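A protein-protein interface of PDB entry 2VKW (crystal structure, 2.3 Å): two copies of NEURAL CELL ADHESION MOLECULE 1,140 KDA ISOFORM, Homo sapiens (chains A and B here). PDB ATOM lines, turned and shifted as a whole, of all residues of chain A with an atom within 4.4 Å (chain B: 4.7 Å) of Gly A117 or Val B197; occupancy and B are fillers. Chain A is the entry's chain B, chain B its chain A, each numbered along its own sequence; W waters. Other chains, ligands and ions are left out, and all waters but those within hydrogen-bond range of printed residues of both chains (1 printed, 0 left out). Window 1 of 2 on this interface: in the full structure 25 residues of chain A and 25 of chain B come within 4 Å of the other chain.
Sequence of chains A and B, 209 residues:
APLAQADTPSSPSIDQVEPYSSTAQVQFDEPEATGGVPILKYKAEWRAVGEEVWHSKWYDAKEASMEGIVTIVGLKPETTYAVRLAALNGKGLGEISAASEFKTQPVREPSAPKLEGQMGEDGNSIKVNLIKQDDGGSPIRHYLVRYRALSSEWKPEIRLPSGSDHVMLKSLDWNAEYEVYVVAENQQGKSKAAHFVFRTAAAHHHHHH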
ATOM      1  N   LEU A 115      10.738  -2.074  -7.376  1.00  0.00           N
ATOM      2  CA  LEU A 115      10.009  -0.843  -7.609  1.00  0.00           C
ATOM      3  C   LEU A 115       9.175  -0.444  -6.403  1.00  0.00           C
ATOM      4  O   LEU A 115       8.535  -1.277  -5.775  1.00  0.00           O
ATOM      5  CB  LEU A 115       9.145  -0.996  -8.863  1.00  0.00           C
ATOM      6  CG  LEU A 115       9.928  -1.545 -10.065  1.00  0.00           C
ATOM      7  CD1 LEU A 115       8.999  -1.776 -11.260  1.00  0.00           C
ATOM      8  CD2 LEU A 115      11.051  -0.579 -10.425  1.00  0.00           C
ATOM      9  N   GLU A 116       9.201   0.845  -6.081  1.00  0.00           N
ATOM     10  CA  GLU A 116       8.476   1.359  -4.931  1.00  0.00           C
ATOM     11  C   GLU A 116       7.664   2.588  -5.316  1.00  0.00           C
ATOM     12  O   GLU A 116       8.217   3.643  -5.602  1.00  0.00           O
ATOM     13  CB  GLU A 116       9.475   1.695  -3.829  1.00  0.00           C
ATOM     14  CG  GLU A 116       8.893   2.380  -2.620  1.00  0.00           C
ATOM     15  CD  GLU A 116       9.980   2.914  -1.715  1.00  0.00           C
ATOM     16  OE1 GLU A 116      10.558   2.128  -0.938  1.00  0.00           O
ATOM     17  OE2 GLU A 116      10.275   4.123  -1.798  1.00  0.00           O
ATOM     18  N   GLY A 117       6.344   2.439  -5.314  1.00  0.00           N
ATOM     19  CA  GLY A 117       5.468   3.535  -5.683  1.00  0.00           C
ATOM     20  C   GLY A 117       5.362   4.671  -4.684  1.00  0.00           C
ATOM     21  O   GLY A 117       5.441   4.480  -3.466  1.00  0.00           O
ATOM     22  N   GLN A 118       5.176   5.868  -5.218  1.00  0.00           N
ATOM     23  CA  GLN A 118       5.042   7.064  -4.405  1.00  0.00           C
ATOM     24  C   GLN A 118       4.156   8.048  -5.150  1.00  0.00           C
ATOM     25  O   GLN A 118       4.192   8.125  -6.387  1.00  0.00           O
ATOM     26  CB  GLN A 118       6.415   7.692  -4.155  1.00  0.00           C
ATOM     27  CG  GLN A 118       6.389   8.957  -3.316  1.00  0.00           C
ATOM     28  CD  GLN A 118       7.773   9.563  -3.127  1.00  0.00           C
ATOM     29  OE1 GLN A 118       8.796   8.915  -3.398  1.00  0.00           O
ATOM     30  NE2 GLN A 118       7.814  10.804  -2.650  1.00  0.00           N
ATOM     31  N   LYS A 127       5.387   8.451  -8.925  1.00  0.00           N
ATOM     32  CA  LYS A 127       6.843   8.403  -8.873  1.00  0.00           C
ATOM     33  C   LYS A 127       7.247   6.972  -8.535  1.00  0.00           C
ATOM     34  O   LYS A 127       6.977   6.480  -7.440  1.00  0.00           O
ATOM     35  CB  LYS A 127       7.358   9.385  -7.810  1.00  0.00           C
ATOM     36  CG  LYS A 127       8.874   9.419  -7.580  1.00  0.00           C
ATOM     37  CD  LYS A 127       9.226  10.584  -6.646  1.00  0.00           C
ATOM     38  CE  LYS A 127      10.717  10.685  -6.323  1.00  0.00           C
ATOM     39  NZ  LYS A 127      11.083   9.983  -5.044  1.00  0.00           N
ATOM     40  N   PHE A 196       5.188  -3.713 -12.192  1.00  0.00           N
ATOM     41  CA  PHE A 196       4.494  -2.942 -11.179  1.00  0.00           C
ATOM     42  C   PHE A 196       3.115  -2.554 -11.713  1.00  0.00           C
ATOM     43  O   PHE A 196       2.999  -2.028 -12.819  1.00  0.00           O
ATOM     44  CB  PHE A 196       5.347  -1.693 -10.907  1.00  0.00           C
ATOM     45  CG  PHE A 196       4.838  -0.819  -9.816  1.00  0.00           C
ATOM     46  CD1 PHE A 196       4.854  -1.250  -8.501  1.00  0.00           C
ATOM     47  CD2 PHE A 196       4.366   0.456 -10.101  1.00  0.00           C
ATOM     48  CE1 PHE A 196       4.408  -0.421  -7.482  1.00  0.00           C
ATOM     49  CE2 PHE A 196       3.916   1.293  -9.093  1.00  0.00           C
ATOM     50  CZ  PHE A 196       3.937   0.855  -7.779  1.00  0.00           C
ATOM     51  N   MET B 119      -2.226   5.317  -4.801  1.00  0.00           N
ATOM     52  CA  MET B 119      -1.651   6.324  -3.910  1.00  0.00           C
ATOM     53  C   MET B 119      -2.685   7.345  -3.491  1.00  0.00           C
ATOM     54  O   MET B 119      -3.501   7.782  -4.296  1.00  0.00           O
ATOM     55  CB  MET B 119      -0.466   7.042  -4.573  1.00  0.00           C
ATOM     56  CG  MET B 119       0.692   6.135  -4.991  1.00  0.00           C
ATOM     57  SD  MET B 119       1.315   5.064  -3.667  1.00  0.00           S
ATOM     58  CE  MET B 119       0.319   3.609  -3.976  1.00  0.00           C
ATOM     59  N   TYR B 178       7.130   2.192   3.410  1.00  0.00           N
ATOM     60  CA  TYR B 178       6.303   1.149   4.003  1.00  0.00           C
ATOM     61  C   TYR B 178       6.339  -0.178   3.249  1.00  0.00           C
ATOM     62  O   TYR B 178       6.386  -0.201   2.020  1.00  0.00           O
ATOM     63  CB  TYR B 178       4.838   1.600   4.060  1.00  0.00           C
ATOM     64  CG  TYR B 178       4.480   2.532   5.193  1.00  0.00           C
ATOM     65  CD1 TYR B 178       4.716   3.901   5.102  1.00  0.00           C
ATOM     66  CD2 TYR B 178       3.896   2.040   6.359  1.00  0.00           C
ATOM     67  CE1 TYR B 178       4.376   4.757   6.149  1.00  0.00           C
ATOM     68  CE2 TYR B 178       3.555   2.883   7.406  1.00  0.00           C
ATOM     69  CZ  TYR B 178       3.798   4.236   7.298  1.00  0.00           C
ATOM     70  OH  TYR B 178       3.474   5.061   8.341  1.00  0.00           O
ATOM     71  N   GLU B 179       6.330  -1.286   3.981  1.00  0.00           N
ATOM     72  CA  GLU B 179       6.262  -2.581   3.320  1.00  0.00           C
ATOM     73  C   GLU B 179       4.939  -3.211   3.747  1.00  0.00           C
ATOM     74  O   GLU B 179       4.521  -3.093   4.899  1.00  0.00           O
ATOM     75  CB  GLU B 179       7.465  -3.489   3.648  1.00  0.00           C
ATOM     76  CG  GLU B 179       7.758  -3.763   5.106  1.00  0.00           C
ATOM     77  CD  GLU B 179       8.873  -4.802   5.281  1.00  0.00           C
ATOM     78  OE1 GLU B 179       9.349  -4.997   6.421  1.00  0.00           O
ATOM     79  OE2 GLU B 179       9.269  -5.431   4.277  1.00  0.00           O
ATOM     80  N   PHE B 196       4.769  -5.628  -1.272  1.00  0.00           N
ATOM     81  CA  PHE B 196       5.288  -4.526  -2.062  1.00  0.00           C
ATOM     82  C   PHE B 196       5.613  -3.376  -1.120  1.00  0.00           C
ATOM     83  O   PHE B 196       5.119  -3.328   0.006  1.00  0.00           O
ATOM     84  CB  PHE B 196       4.272  -4.092  -3.132  1.00  0.00           C
ATOM     85  CG  PHE B 196       3.108  -3.303  -2.598  1.00  0.00           C
ATOM     86  CD1 PHE B 196       3.127  -1.912  -2.620  1.00  0.00           C
ATOM     87  CD2 PHE B 196       1.989  -3.949  -2.077  1.00  0.00           C
ATOM     88  CE1 PHE B 196       2.049  -1.172  -2.130  1.00  0.00           C
ATOM     89  CE2 PHE B 196       0.905  -3.220  -1.583  1.00  0.00           C
ATOM     90  CZ  PHE B 196       0.934  -1.827  -1.611  1.00  0.00           C
ATOM     91  N   VAL B 197       6.472  -2.473  -1.578  1.00  0.00           N
ATOM     92  CA  VAL B 197       6.870  -1.316  -0.795  1.00  0.00           C
ATOM     93  C   VAL B 197       6.389  -0.044  -1.480  1.00  0.00           C
ATOM     94  O   VAL B 197       6.282   0.003  -2.710  1.00  0.00           O
ATOM     95  CB  VAL B 197       8.401  -1.254  -0.649  1.00  0.00           C
ATOM     96  CG1 VAL B 197       8.887  -2.393   0.238  1.00  0.00           C
ATOM     97  CG2 VAL B 197       9.054  -1.352  -2.024  1.00  0.00           C
ATOM     98  N   PHE B 198       6.093   0.982  -0.687  1.00  0.00           N
ATOM     99  CA  PHE B 198       5.641   2.265  -1.220  1.00  0.00           C
ATOM    100  C   PHE B 198       6.148   3.367  -0.297  1.00  0.00           C
ATOM    101  O   PHE B 198       6.559   3.088   0.829  1.00  0.00           O
ATOM    102  CB  PHE B 198       4.104   2.293  -1.333  1.00  0.00           C
ATOM    103  CG  PHE B 198       3.389   2.431  -0.014  1.00  0.00           C
ATOM    104  CD1 PHE B 198       3.072   3.686   0.491  1.00  0.00           C
ATOM    105  CD2 PHE B 198       3.025   1.304   0.716  1.00  0.00           C
ATOM    106  CE1 PHE B 198       2.403   3.817   1.707  1.00  0.00           C
ATOM    107  CE2 PHE B 198       2.357   1.420   1.931  1.00  0.00           C
ATOM    108  CZ  PHE B 198       2.045   2.681   2.429  1.00  0.00           C
ATOM    109  N   ARG B 199       6.135   4.611  -0.764  1.00  0.00           N
ATOM    110  CA  ARG B 199       6.634   5.722   0.047  1.00  0.00           C
ATOM    111  C   ARG B 199       5.639   6.864   0.179  1.00  0.00           C
ATOM    112  O   ARG B 199       5.042   7.307  -0.805  1.00  0.00           O
ATOM    113  CB  ARG B 199       7.939   6.261  -0.552  1.00  0.00           C
ATOM    114  CG  ARG B 199       8.610   7.347   0.266  1.00  0.00           C
ATOM    115  CD  ARG B 199       9.833   7.904  -0.449  1.00  0.00           C
ATOM    116  NE  ARG B 199      10.711   6.850  -0.958  1.00  0.00           N
ATOM    117  CZ  ARG B 199      11.743   7.066  -1.768  1.00  0.00           C
ATOM    118  NH1 ARG B 199      12.026   8.302  -2.153  1.00  0.00           N
ATOM    119  NH2 ARG B 199      12.479   6.053  -2.212  1.00  0.00           N
HETATM  120  O   HOH W   1       4.797   0.134  -4.797  1.00  0.00           O
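NZ of Lys A127 lies close to NH1 of Arg B199 (3.5 Å). NE of Arg B199 lies within salt-bridge range of OE2 of Glu A116 (2.9 Å). O of Gly A117 is in hydrogen-bond range of N of Arg B199 (2.8 Å).
The backbone NH (N) of Tyr B178 sits at hydrogen-bond distance from the backbone carbonyl oxygen (O) of Phe B198, 2.8 Å away. The backbone carbonyl oxygen (O) of Gln A118 sits at hydrogen-bond distance from the backbone NH (N) of Lys A127 (2.8 Å).
Among the printed residues, merely in contact across the chains: Gly A117 with Phe B198 (3.2 Å), Gln A118 with Arg B199 (3.3 Å), Glu A116 with Val B197 (3.4 Å), Glu A116 with Phe B198 (3.5 Å), Gly A117 with Val B197 (3.6 Å), Leu A115 with Val B197 (3.8 Å) and Gln A118 with Met B119 (3.96 Å).
Of the printed residues of chain B, Leu A115 touches Val B197. Printed residues of chain B within 4 Å of Glu A116: Val B197, Phe B198 and Arg B199. Gly A117 touches just these residues of chain B: Val B197 (3.6 Å), Phe B198 (3.2 Å) and Arg B199 (2.8 Å). Of the printed residues of chain B, Gln A118 touches Met B119 and Arg B199. Tyr B178 touches none of the printed residues of chain A. Of chain A, only Leu A115 (3.8 Å), Glu A116 (3.4 Å) and Gly A117 (3.6 Å) come within 4 Å of Val B197. Of the printed residues of chain A, Arg B199 touches Glu A116, Gly A117, Gln A118 and Lys A127. The nearest residue of chain B that does not touch Gly A117 is Met B119 (4.2 Å). The nearest printed residue of chain A that does not touch Val B197 is Phe A196 (5.1 Å). The nearest printed residue of chain B that does not touch Glu A116 is Tyr B178 (5.5 Å).
Among the printed residues, 10 pairs touch across the chains. Among the printed residues, Asp or Glu carboxylates within 4 Å of a Lys or Arg side-chain nitrogen of the other chain: Glu A116 with Arg B199 (2.9 Å).
1 position is printed for both chains. Of the 10 pairs that touch across the chains among the printed residues, none has its exchanged pair printed and touching as well.
Water W1 bridges the backbone carbonyl oxygen of Val B197 (2.6 Å) and the backbone NH of Gly A117 (2.8 Å).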
